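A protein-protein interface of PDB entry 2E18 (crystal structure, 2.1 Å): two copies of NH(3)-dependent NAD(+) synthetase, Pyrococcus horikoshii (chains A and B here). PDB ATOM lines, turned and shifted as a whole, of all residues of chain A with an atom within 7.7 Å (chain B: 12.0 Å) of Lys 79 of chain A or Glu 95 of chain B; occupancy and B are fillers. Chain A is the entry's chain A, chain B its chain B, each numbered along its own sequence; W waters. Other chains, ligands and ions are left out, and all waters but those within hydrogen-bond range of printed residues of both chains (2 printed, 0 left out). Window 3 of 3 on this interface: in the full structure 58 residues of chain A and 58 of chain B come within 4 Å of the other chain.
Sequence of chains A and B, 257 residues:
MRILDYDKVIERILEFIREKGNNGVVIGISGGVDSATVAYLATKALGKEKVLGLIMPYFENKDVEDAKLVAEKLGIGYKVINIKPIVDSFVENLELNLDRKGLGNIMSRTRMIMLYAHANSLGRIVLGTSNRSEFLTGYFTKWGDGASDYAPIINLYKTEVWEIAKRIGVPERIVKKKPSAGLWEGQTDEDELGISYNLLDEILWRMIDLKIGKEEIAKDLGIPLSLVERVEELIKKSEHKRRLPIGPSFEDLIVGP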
ATOM      1  N   ILE A  27     -14.808 -25.724  30.219  1.00  0.00           N
ATOM      2  CA  ILE A  27     -14.025 -24.615  29.705  1.00  0.00           C
ATOM      3  C   ILE A  27     -14.676 -23.964  28.493  1.00  0.00           C
ATOM      4  O   ILE A  27     -15.293 -24.637  27.666  1.00  0.00           O
ATOM      5  CB  ILE A  27     -12.626 -25.095  29.271  1.00  0.00           C
ATOM      6  CG1 ILE A  27     -11.970 -25.903  30.396  1.00  0.00           C
ATOM      7  CG2 ILE A  27     -11.743 -23.896  28.944  1.00  0.00           C
ATOM      8  CD1 ILE A  27     -10.679 -26.601  29.971  1.00  0.00           C
ATOM      9  N   ILE A  29     -14.336 -22.527  25.026  1.00  0.00           N
ATOM     10  CA  ILE A  29     -13.410 -22.574  23.900  1.00  0.00           C
ATOM     11  C   ILE A  29     -13.857 -21.644  22.763  1.00  0.00           C
ATOM     12  O   ILE A  29     -14.939 -21.774  22.201  1.00  0.00           O
ATOM     13  CB  ILE A  29     -13.324 -24.022  23.418  1.00  0.00           C
ATOM     14  CG1 ILE A  29     -12.805 -24.927  24.540  1.00  0.00           C
ATOM     15  CG2 ILE A  29     -12.332 -24.126  22.249  1.00  0.00           C
ATOM     16  CD1 ILE A  29     -12.644 -26.376  24.075  1.00  0.00           C
ATOM     17  N   LEU A  52     -15.002 -30.802  29.296  1.00  0.00           N
ATOM     18  CA  LEU A  52     -16.144 -30.451  28.466  1.00  0.00           C
ATOM     19  C   LEU A  52     -15.901 -29.030  27.968  1.00  0.00           C
ATOM     20  O   LEU A  52     -15.669 -28.111  28.765  1.00  0.00           O
ATOM     21  CB  LEU A  52     -17.457 -30.492  29.253  1.00  0.00           C
ATOM     22  CG  LEU A  52     -18.662 -29.993  28.435  1.00  0.00           C
ATOM     23  CD1 LEU A  52     -18.954 -30.956  27.264  1.00  0.00           C
ATOM     24  CD2 LEU A  52     -19.880 -29.867  29.336  1.00  0.00           C
ATOM     25  N   GLY A  53     -15.933 -28.856  26.653  1.00  0.00           N
ATOM     26  CA  GLY A  53     -15.717 -27.536  26.094  1.00  0.00           C
ATOM     27  C   GLY A  53     -16.997 -26.900  25.576  1.00  0.00           C
ATOM     28  O   GLY A  53     -17.769 -27.536  24.868  1.00  0.00           O
ATOM     29  N   LEU A  54     -17.241 -25.647  25.934  1.00  0.00           N
ATOM     30  CA  LEU A  54     -18.428 -24.970  25.426  1.00  0.00           C
ATOM     31  C   LEU A  54     -17.970 -23.917  24.419  1.00  0.00           C
ATOM     32  O   LEU A  54     -17.149 -23.050  24.729  1.00  0.00           O
ATOM     33  CB  LEU A  54     -19.232 -24.315  26.556  1.00  0.00           C
ATOM     34  CG  LEU A  54     -19.767 -25.208  27.686  1.00  0.00           C
ATOM     35  CD1 LEU A  54     -20.622 -24.361  28.598  1.00  0.00           C
ATOM     36  CD2 LEU A  54     -20.586 -26.364  27.144  1.00  0.00           C
ATOM     37  N   ILE A  55     -18.473 -24.035  23.197  1.00  0.00           N
ATOM     38  CA  ILE A  55     -18.160 -23.092  22.129  1.00  0.00           C
ATOM     39  C   ILE A  55     -19.434 -22.264  22.066  1.00  0.00           C
ATOM     40  O   ILE A  55     -20.499 -22.785  21.725  1.00  0.00           O
ATOM     41  CB  ILE A  55     -17.894 -23.850  20.810  1.00  0.00           C
ATOM     42  CG1 ILE A  55     -16.729 -24.834  21.032  1.00  0.00           C
ATOM     43  CG2 ILE A  55     -17.582 -22.871  19.685  1.00  0.00           C
ATOM     44  CD1 ILE A  55     -16.328 -25.629  19.796  1.00  0.00           C
ATOM     45  N   MET A  56     -19.337 -20.987  22.426  1.00  0.00           N
ATOM     46  CA  MET A  56     -20.521 -20.132  22.493  1.00  0.00           C
ATOM     47  C   MET A  56     -20.463 -18.906  21.592  1.00  0.00           C
ATOM     48  O   MET A  56     -20.241 -17.782  22.047  1.00  0.00           O
ATOM     49  CB  MET A  56     -20.734 -19.716  23.953  1.00  0.00           C
ATOM     50  CG  MET A  56     -20.808 -20.918  24.891  1.00  0.00           C
ATOM     51  SD  MET A  56     -20.530 -20.552  26.632  1.00  0.00           S
ATOM     52  CE  MET A  56     -18.757 -20.387  26.676  1.00  0.00           C
ATOM     53  N   PRO A  57     -20.696 -19.106  20.292  1.00  0.00           N
ATOM     54  CA  PRO A  57     -20.602 -17.981  19.358  1.00  0.00           C
ATOM     55  C   PRO A  57     -21.784 -17.009  19.479  1.00  0.00           C
ATOM     56  O   PRO A  57     -22.901 -17.385  19.792  1.00  0.00           O
ATOM     57  CB  PRO A  57     -20.591 -18.555  17.946  1.00  0.00           C
ATOM     58  CG  PRO A  57     -21.241 -19.930  18.021  1.00  0.00           C
ATOM     59  CD  PRO A  57     -20.891 -20.335  19.525  1.00  0.00           C
ATOM     60  N   ALA A  71     -11.497 -28.531  19.765  1.00  0.00           N
ATOM     61  CA  ALA A  71     -12.306 -29.584  20.363  1.00  0.00           C
ATOM     62  C   ALA A  71     -12.072 -30.912  19.657  1.00  0.00           C
ATOM     63  O   ALA A  71     -11.933 -31.950  20.299  1.00  0.00           O
ATOM     64  CB  ALA A  71     -13.786 -29.214  20.288  1.00  0.00           C
ATOM     65  N   ILE A  76     -12.212 -34.131  23.067  1.00  0.00           N
ATOM     66  CA  ILE A  76     -13.029 -33.840  24.238  1.00  0.00           C
ATOM     67  C   ILE A  76     -14.515 -33.748  23.891  1.00  0.00           C
ATOM     68  O   ILE A  76     -14.895 -33.652  22.725  1.00  0.00           O
ATOM     69  CB  ILE A  76     -12.625 -32.487  24.895  1.00  0.00           C
ATOM     70  CG1 ILE A  76     -12.846 -31.341  23.899  1.00  0.00           C
ATOM     71  CG2 ILE A  76     -11.160 -32.532  25.359  1.00  0.00           C
ATOM     72  CD1 ILE A  76     -12.800 -29.937  24.529  1.00  0.00           C
ATOM     73  N   GLY A  77     -15.360 -33.791  24.912  1.00  0.00           N
ATOM     74  CA  GLY A  77     -16.779 -33.637  24.670  1.00  0.00           C
ATOM     75  C   GLY A  77     -16.941 -32.136  24.498  1.00  0.00           C
ATOM     76  O   GLY A  77     -16.201 -31.367  25.112  1.00  0.00           O
ATOM     77  N   TYR A  78     -17.862 -31.700  23.646  1.00  0.00           N
ATOM     78  CA  TYR A  78     -18.069 -30.270  23.470  1.00  0.00           C
ATOM     79  C   TYR A  78     -19.488 -29.978  23.024  1.00  0.00           C
ATOM     80  O   TYR A  78     -20.211 -30.874  22.579  1.00  0.00           O
ATOM     81  CB  TYR A  78     -17.050 -29.687  22.482  1.00  0.00           C
ATOM     82  CG  TYR A  78     -17.254 -30.079  21.040  1.00  0.00           C
ATOM     83  CD1 TYR A  78     -16.693 -31.254  20.529  1.00  0.00           C
ATOM     84  CD2 TYR A  78     -17.989 -29.267  20.180  1.00  0.00           C
ATOM     85  CE1 TYR A  78     -16.852 -31.608  19.187  1.00  0.00           C
ATOM     86  CE2 TYR A  78     -18.157 -29.609  18.836  1.00  0.00           C
ATOM     87  CZ  TYR A  78     -17.582 -30.780  18.349  1.00  0.00           C
ATOM     88  OH  TYR A  78     -17.732 -31.108  17.023  1.00  0.00           O
ATOM     89  N   LYS A  79     -19.878 -28.715  23.156  1.00  0.00           N
ATOM     90  CA  LYS A  79     -21.221 -28.273  22.823  1.00  0.00           C
ATOM     91  C   LYS A  79     -21.155 -26.873  22.201  1.00  0.00           C
ATOM     92  O   LYS A  79     -20.487 -25.991  22.736  1.00  0.00           O
ATOM     93  CB  LYS A  79     -22.032 -28.250  24.123  1.00  0.00           C
ATOM     94  CG  LYS A  79     -23.510 -28.003  24.031  1.00  0.00           C
ATOM     95  CD  LYS A  79     -24.061 -28.033  25.459  1.00  0.00           C
ATOM     96  CE  LYS A  79     -25.562 -28.215  25.522  1.00  0.00           C
ATOM     97  NZ  LYS A  79     -25.970 -28.267  26.961  1.00  0.00           N
ATOM     98  N   VAL A  80     -21.826 -26.682  21.066  1.00  0.00           N
ATOM     99  CA  VAL A  80     -21.861 -25.377  20.403  1.00  0.00           C
ATOM    100  C   VAL A  80     -23.177 -24.727  20.841  1.00  0.00           C
ATOM    101  O   VAL A  80     -24.272 -25.270  20.628  1.00  0.00           O
ATOM    102  CB  VAL A  80     -21.822 -25.515  18.861  1.00  0.00           C
ATOM    103  CG1 VAL A  80     -21.793 -24.142  18.202  1.00  0.00           C
ATOM    104  CG2 VAL A  80     -20.582 -26.282  18.441  1.00  0.00           C
ATOM    105  N   ILE A  81     -23.060 -23.576  21.491  1.00  0.00           N
ATOM    106  CA  ILE A  81     -24.232 -22.865  21.994  1.00  0.00           C
ATOM    107  C   ILE A  81     -24.329 -21.452  21.426  1.00  0.00           C
ATOM    108  O   ILE A  81     -23.513 -20.591  21.741  1.00  0.00           O
ATOM    109  CB  ILE A  81     -24.194 -22.741  23.536  1.00  0.00           C
ATOM    110  CG1 ILE A  81     -24.030 -24.121  24.169  1.00  0.00           C
ATOM    111  CG2 ILE A  81     -25.492 -22.072  24.045  1.00  0.00           C
ATOM    112  CD1 ILE A  81     -23.815 -24.073  25.680  1.00  0.00           C
ATOM    113  N   ASN A  82     -25.335 -21.225  20.594  1.00  0.00           N
ATOM    114  CA  ASN A  82     -25.567 -19.910  20.008  1.00  0.00           C
ATOM    115  C   ASN A  82     -26.116 -19.006  21.122  1.00  0.00           C
ATOM    116  O   ASN A  82     -27.206 -19.247  21.628  1.00  0.00           O
ATOM    117  CB  ASN A  82     -26.586 -20.044  18.869  1.00  0.00           C
ATOM    118  CG  ASN A  82     -27.001 -18.707  18.296  1.00  0.00           C
ATOM    119  OD1 ASN A  82     -26.327 -17.685  18.497  1.00  0.00           O
ATOM    120  ND2 ASN A  82     -28.111 -18.704  17.557  1.00  0.00           N
ATOM    121  N   MET A 114     -23.463 -19.630  31.263  1.00  0.00           N
ATOM    122  CA  MET A 114     -23.520 -20.917  30.567  1.00  0.00           C
ATOM    123  C   MET A 114     -22.486 -21.884  31.133  1.00  0.00           C
ATOM    124  O   MET A 114     -22.802 -23.033  31.406  1.00  0.00           O
ATOM    125  CB  MET A 114     -23.256 -20.738  29.070  1.00  0.00           C
ATOM    126  CG  MET A 114     -24.435 -20.224  28.269  1.00  0.00           C
ATOM    127  SD  MET A 114     -25.770 -21.443  28.149  1.00  0.00           S
ATOM    128  CE  MET A 114     -27.013 -20.422  27.424  1.00  0.00           C
ATOM    129  N   HIS A 118     -23.392 -25.376  33.372  1.00  0.00           N
ATOM    130  CA  HIS A 118     -22.938 -26.715  33.025  1.00  0.00           C
ATOM    131  C   HIS A 118     -22.062 -27.347  34.113  1.00  0.00           C
ATOM    132  O   HIS A 118     -22.222 -28.519  34.436  1.00  0.00           O
ATOM    133  CB  HIS A 118     -22.187 -26.699  31.693  1.00  0.00           C
ATOM    134  CG  HIS A 118     -23.088 -26.610  30.500  1.00  0.00           C
ATOM    135  ND1 HIS A 118     -23.809 -25.475  30.189  1.00  0.00           N
ATOM    136  CD2 HIS A 118     -23.422 -27.535  29.569  1.00  0.00           C
ATOM    137  CE1 HIS A 118     -24.552 -25.706  29.120  1.00  0.00           C
ATOM    138  NE2 HIS A 118     -24.336 -26.950  28.723  1.00  0.00           N
ATOM    139  N   SER A 121     -24.267 -28.333  37.044  1.00  0.00           N
ATOM    140  CA  SER A 121     -25.035 -29.532  36.741  1.00  0.00           C
ATOM    141  C   SER A 121     -24.165 -30.777  36.814  1.00  0.00           C
ATOM    142  O   SER A 121     -24.575 -31.798  37.366  1.00  0.00           O
ATOM    143  CB  SER A 121     -25.647 -29.436  35.339  1.00  0.00           C
ATOM    144  OG  SER A 121     -26.380 -30.608  35.028  1.00  0.00           O
ATOM    145  N   ILE B  86     -35.584 -15.259  30.343  1.00  0.00           N
ATOM    146  CA  ILE B  86     -34.143 -15.376  30.114  1.00  0.00           C
ATOM    147  C   ILE B  86     -33.539 -16.517  30.929  1.00  0.00           C
ATOM    148  O   ILE B  86     -32.716 -17.281  30.418  1.00  0.00           O
ATOM    149  CB  ILE B  86     -33.402 -14.057  30.447  1.00  0.00           C
ATOM    150  CG1 ILE B  86     -33.644 -13.042  29.323  1.00  0.00           C
ATOM    151  CG2 ILE B  86     -31.905 -14.322  30.624  1.00  0.00           C
ATOM    152  CD1 ILE B  86     -32.917 -11.715  29.514  1.00  0.00           C
ATOM    153  N   VAL B  87     -33.946 -16.638  32.188  1.00  0.00           N
ATOM    154  CA  VAL B  87     -33.431 -17.704  33.038  1.00  0.00           C
ATOM    155  C   VAL B  87     -33.821 -19.071  32.462  1.00  0.00           C
ATOM    156  O   VAL B  87     -32.994 -19.987  32.393  1.00  0.00           O
ATOM    157  CB  VAL B  87     -33.969 -17.578  34.485  1.00  0.00           C
ATOM    158  CG1 VAL B  87     -33.626 -18.837  35.284  1.00  0.00           C
ATOM    159  CG2 VAL B  87     -33.372 -16.349  35.158  1.00  0.00           C
ATOM    160  N   ASP B  88     -35.070 -19.212  32.036  1.00  0.00           N
ATOM    161  CA  ASP B  88     -35.509 -20.479  31.475  1.00  0.00           C
ATOM    162  C   ASP B  88     -34.797 -20.797  30.163  1.00  0.00           C
ATOM    163  O   ASP B  88     -34.596 -21.965  29.830  1.00  0.00           O
ATOM    164  CB  ASP B  88     -37.028 -20.478  31.272  1.00  0.00           C
ATOM    165  CG  ASP B  88     -37.788 -20.512  32.587  1.00  0.00           C
ATOM    166  OD1 ASP B  88     -37.182 -20.854  33.628  1.00  0.00           O
ATOM    167  OD2 ASP B  88     -38.994 -20.208  32.576  1.00  0.00           O
ATOM    168  N   SER B  89     -34.402 -19.768  29.419  1.00  0.00           N
ATOM    169  CA  SER B  89     -33.689 -20.005  28.170  1.00  0.00           C
ATOM    170  C   SER B  89     -32.302 -20.590  28.455  1.00  0.00           C
ATOM    171  O   SER B  89     -31.815 -21.450  27.708  1.00  0.00           O
ATOM    172  CB  SER B  89     -33.558 -18.709  27.369  1.00  0.00           C
ATOM    173  OG  SER B  89     -32.915 -18.976  26.137  1.00  0.00           O
ATOM    174  N   PHE B  90     -31.665 -20.121  29.529  1.00  0.00           N
ATOM    175  CA  PHE B  90     -30.347 -20.634  29.924  1.00  0.00           C
ATOM    176  C   PHE B  90     -30.526 -22.120  30.228  1.00  0.00           C
ATOM    177  O   PHE B  90     -29.755 -22.964  29.768  1.00  0.00           O
ATOM    178  CB  PHE B  90     -29.821 -19.933  31.196  1.00  0.00           C
ATOM    179  CG  PHE B  90     -29.002 -18.699  30.925  1.00  0.00           C
ATOM    180  CD1 PHE B  90     -27.788 -18.786  30.235  1.00  0.00           C
ATOM    181  CD2 PHE B  90     -29.457 -17.445  31.321  1.00  0.00           C
ATOM    182  CE1 PHE B  90     -27.044 -17.647  29.938  1.00  0.00           C
ATOM    183  CE2 PHE B  90     -28.716 -16.283  31.028  1.00  0.00           C
ATOM    184  CZ  PHE B  90     -27.514 -16.382  30.339  1.00  0.00           C
ATOM    185  N   VAL B  91     -31.548 -22.422  31.021  1.00  0.00           N
ATOM    186  CA  VAL B  91     -31.856 -23.795  31.396  1.00  0.00           C
ATOM    187  C   VAL B  91     -32.136 -24.653  30.156  1.00  0.00           C
ATOM    188  O   VAL B  91     -31.683 -25.792  30.081  1.00  0.00           O
ATOM    189  CB  VAL B  91     -33.084 -23.839  32.338  1.00  0.00           C
ATOM    190  CG1 VAL B  91     -33.392 -25.274  32.750  1.00  0.00           C
ATOM    191  CG2 VAL B  91     -32.811 -22.988  33.559  1.00  0.00           C
ATOM    192  N   GLU B  92     -32.884 -24.109  29.192  1.00  0.00           N
ATOM    193  CA  GLU B  92     -33.206 -24.839  27.963  1.00  0.00           C
ATOM    194  C   GLU B  92     -31.956 -25.173  27.167  1.00  0.00           C
ATOM    195  O   GLU B  92     -31.852 -26.254  26.586  1.00  0.00           O
ATOM    196  CB  GLU B  92     -34.173 -24.033  27.093  1.00  0.00           C
ATOM    197  CG  GLU B  92     -35.625 -24.207  27.490  1.00  0.00           C
ATOM    198  CD  GLU B  92     -36.486 -23.037  27.067  1.00  0.00           C
ATOM    199  OE1 GLU B  92     -36.212 -22.454  25.992  1.00  0.00           O
ATOM    200  OE2 GLU B  92     -37.443 -22.709  27.806  1.00  0.00           O
ATOM    201  N   ASN B  93     -31.009 -24.243  27.141  1.00  0.00           N
ATOM    202  CA  ASN B  93     -29.760 -24.466  26.435  1.00  0.00           C
ATOM    203  C   ASN B  93     -28.931 -25.480  27.225  1.00  0.00           C
ATOM    204  O   ASN B  93     -28.216 -26.291  26.645  1.00  0.00           O
ATOM    205  CB  ASN B  93     -28.992 -23.145  26.275  1.00  0.00           C
ATOM    206  CG  ASN B  93     -29.458 -22.347  25.074  1.00  0.00           C
ATOM    207  OD1 ASN B  93     -29.095 -22.645  23.935  1.00  0.00           O
ATOM    208  ND2 ASN B  93     -30.283 -21.342  25.318  1.00  0.00           N
ATOM    209  N   LEU B  94     -29.049 -25.449  28.547  1.00  0.00           N
ATOM    210  CA  LEU B  94     -28.302 -26.382  29.391  1.00  0.00           C
ATOM    211  C   LEU B  94     -28.622 -27.835  29.020  1.00  0.00           C
ATOM    212  O   LEU B  94     -27.720 -28.654  28.863  1.00  0.00           O
ATOM    213  CB  LEU B  94     -28.624 -26.133  30.869  1.00  0.00           C
ATOM    214  CG  LEU B  94     -27.939 -27.027  31.917  1.00  0.00           C
ATOM    215  CD1 LEU B  94     -26.424 -26.844  31.866  1.00  0.00           C
ATOM    216  CD2 LEU B  94     -28.466 -26.668  33.300  1.00  0.00           C
ATOM    217  N   GLU B  95     -29.909 -28.140  28.892  1.00  0.00           N
ATOM    218  CA  GLU B  95     -30.379 -29.479  28.525  1.00  0.00           C
ATOM    219  C   GLU B  95     -29.933 -30.547  29.505  1.00  0.00           C
ATOM    220  O   GLU B  95     -29.734 -31.704  29.143  1.00  0.00           O
ATOM    221  CB  GLU B  95     -29.899 -29.844  27.123  1.00  0.00           C
ATOM    222  CG  GLU B  95     -30.337 -28.855  26.062  1.00  0.00           C
ATOM    223  CD  GLU B  95     -29.746 -29.157  24.705  1.00  0.00           C
ATOM    224  OE1 GLU B  95     -28.555 -29.538  24.637  1.00  0.00           O
ATOM    225  OE2 GLU B  95     -30.468 -28.996  23.699  1.00  0.00           O
ATOM    226  N   LEU B  96     -29.758 -30.137  30.748  1.00  0.00           N
ATOM    227  CA  LEU B  96     -29.355 -31.039  31.804  1.00  0.00           C
ATOM    228  C   LEU B  96     -30.162 -30.612  33.003  1.00  0.00           C
ATOM    229  O   LEU B  96     -30.813 -29.550  32.998  1.00  0.00           O
ATOM    230  CB  LEU B  96     -27.863 -30.894  32.138  1.00  0.00           C
ATOM    231  CG  LEU B  96     -26.828 -31.367  31.110  1.00  0.00           C
ATOM    232  CD1 LEU B  96     -25.424 -30.948  31.569  1.00  0.00           C
ATOM    233  CD2 LEU B  96     -26.915 -32.884  30.950  1.00  0.00           C
ATOM    234  N   ASN B  97     -30.121 -31.447  34.030  1.00  0.00           N
ATOM    235  CA  ASN B  97     -30.796 -31.150  35.266  1.00  0.00           C
ATOM    236  C   ASN B  97     -30.011 -30.093  36.007  1.00  0.00           C
ATOM    237  O   ASN B  97     -28.808 -29.945  35.841  1.00  0.00           O
ATOM    238  CB  ASN B  97     -30.858 -32.431  36.099  1.00  0.00           C
ATOM    239  CG  ASN B  97     -31.920 -33.341  35.540  1.00  0.00           C
ATOM    240  OD1 ASN B  97     -31.664 -34.478  35.153  1.00  0.00           O
ATOM    241  ND2 ASN B  97     -33.156 -32.814  35.501  1.00  0.00           N
ATOM    242  N   LEU B  98     -30.687 -29.334  36.855  1.00  0.00           N
ATOM    243  CA  LEU B  98     -30.033 -28.308  37.658  1.00  0.00           C
ATOM    244  C   LEU B  98     -30.828 -28.245  38.957  1.00  0.00           C
ATOM    245  O   LEU B  98     -32.053 -28.128  38.923  1.00  0.00           O
ATOM    246  CB  LEU B  98     -30.091 -26.957  36.931  1.00  0.00           C
ATOM    247  CG  LEU B  98     -29.244 -25.796  37.458  1.00  0.00           C
ATOM    248  CD1 LEU B  98     -27.767 -26.193  37.479  1.00  0.00           C
ATOM    249  CD2 LEU B  98     -29.441 -24.588  36.558  1.00  0.00           C
ATOM    250  N   ASP B  99     -30.163 -28.349  40.100  1.00  0.00           N
ATOM    251  CA  ASP B  99     -30.924 -28.283  41.343  1.00  0.00           C
ATOM    252  C   ASP B  99     -31.354 -26.840  41.597  1.00  0.00           C
ATOM    253  O   ASP B  99     -30.981 -25.930  40.847  1.00  0.00           O
ATOM    254  CB  ASP B  99     -30.128 -28.835  42.532  1.00  0.00           C
ATOM    255  CG  ASP B  99     -28.845 -28.088  42.780  1.00  0.00           C
ATOM    256  OD1 ASP B  99     -28.793 -26.867  42.517  1.00  0.00           O
ATOM    257  OD2 ASP B  99     -27.889 -28.731  43.261  1.00  0.00           O
ATOM    258  N   LEU B 103     -30.110 -23.223  39.790  1.00  0.00           N
ATOM    259  CA  LEU B 103     -31.096 -22.386  39.110  1.00  0.00           C
ATOM    260  C   LEU B 103     -31.117 -21.010  39.766  1.00  0.00           C
ATOM    261  O   LEU B 103     -31.243 -19.990  39.094  1.00  0.00           O
ATOM    262  CB  LEU B 103     -32.493 -23.017  39.204  1.00  0.00           C
ATOM    263  CG  LEU B 103     -33.614 -22.212  38.548  1.00  0.00           C
ATOM    264  CD1 LEU B 103     -33.322 -22.066  37.056  1.00  0.00           C
ATOM    265  CD2 LEU B 103     -34.956 -22.906  38.764  1.00  0.00           C
ATOM    266  N   ILE B 106     -28.408 -18.922  38.401  1.00  0.00           N
ATOM    267  CA  ILE B 106     -28.638 -18.356  37.075  1.00  0.00           C
ATOM    268  C   ILE B 106     -29.442 -17.068  37.251  1.00  0.00           C
ATOM    269  O   ILE B 106     -29.186 -16.068  36.583  1.00  0.00           O
ATOM    270  CB  ILE B 106     -29.416 -19.321  36.151  1.00  0.00           C
ATOM    271  CG1 ILE B 106     -28.528 -20.520  35.790  1.00  0.00           C
ATOM    272  CG2 ILE B 106     -29.863 -18.568  34.853  1.00  0.00           C
ATOM    273  CD1 ILE B 106     -29.229 -21.606  34.971  1.00  0.00           C
HETATM  274  O   HOH W   1     -29.008 -21.291  21.716  1.00  0.00           O
HETATM  275  O   HOH W   2     -26.410 -31.446  26.262  1.00  0.00           O
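Hydrophobic or aromatic side chains of chain A that line the printed part of chain B: Ile 81, Met 114 and His 118.
Water W1 bridges OD1 of Asn 93 of chain B and O of Asn 82 of chain A.
Water W2 lies within hydrogen-bond range of NZ of Lys 79 of chain A (3.3 Å) and OE1 of Glu 95 of chain B (3.3 Å).
Of chain A, only Lys 79 comes within 4 Å of Glu 95 of chain B.
No residue of chain B comes within 4 Å of Gly 53 of chain A.
No residue of chain B comes within 4 Å of Leu 54 of chain A.
No residue of chain B comes within 4 Å of Ile 55 of chain A.
No residue of chain B comes within 4 Å of Gly 77 of chain A.
No residue of chain B comes within 4 Å of Tyr 78 of chain A.
Of the printed residues of chain B, Ile 81 of chain A touches Asn 93.
Printed residues of chain A within 4 Å of Leu 94 of chain B: Lys 79 (2.6 Å) and His 118 (3.4 Å).
Of the printed residues of chain B, His 118 of chain A touches Leu 94.
Printed residues of chain A within 4 Å of Leu 96 of chain B: Ser 121 (3.3 Å).
Ala 71 of chain A touches none of the printed residues of chain B.
The nearest printed residue of chain B that does not touch Ser 121 of chain A is Leu 98 of chain B (4.1 Å).
N of Lys 79 of chain A lies within hydrogen-bond range of O of Gly 53 of chain A (3.0 Å).
NZ of Lys 79 of chain A lies within hydrogen-bond range of NE2 of His 118 of chain A, at 2.7 Å.
A ring nitrogen (ND1) of His 118 of chain A lies within hydrogen-bond range of the backbone carbonyl oxygen (O) of Met 114 of chain A (2.9 Å).
The backbone carbonyl oxygen of Ile 55 of chain A sits at hydrogen-bond distance from the backbone NH of Ile 81 of chain A (2.7 Å).
The side-chain amide nitrogen of Asn 93 of chain B lies within hydrogen-bond range of the backbone carbonyl oxygen of Ser 89 of chain B, 2.8 Å away.
O of Lys 79 of chain A sits at hydrogen-bond distance from N of Ile 55 of chain A (2.8 Å).
The side-chain amino group of Lys 79 of chain A is in salt-bridge range of the side-chain carboxylate of Glu 95 of chain B, 3.7 Å away.
The side-chain hydroxyl (OG) of Ser 121 of chain A sits at hydrogen-bond distance from the backbone carbonyl oxygen (O) of Asn 97 of chain B, at 2.6 Å.
The side-chain amino group of Lys 79 of chain A sits at hydrogen-bond distance from the backbone carbonyl oxygen of Asn 93 of chain B, at 3.0 Å.
The side-chain amino group (NZ) of Lys 79 of chain A is in hydrogen-bond range of the backbone carbonyl oxygen (O) of Leu 94 of chain B (2.6 Å).
Among the printed residues, merely in contact across the chains: Ser 121 of chain A with Leu 96 of chain B (3.3 Å), Met 114 of chain A with Phe 90 of chain B (3.3 Å), His 118 of chain A with Leu 94 of chain B (3.4 Å), Met 114 of chain A with Asn 93 of chain B (3.6 Å) and Ile 81 of chain A with Asn 93 of chain B (3.6 Å).
No position is printed for both chains.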
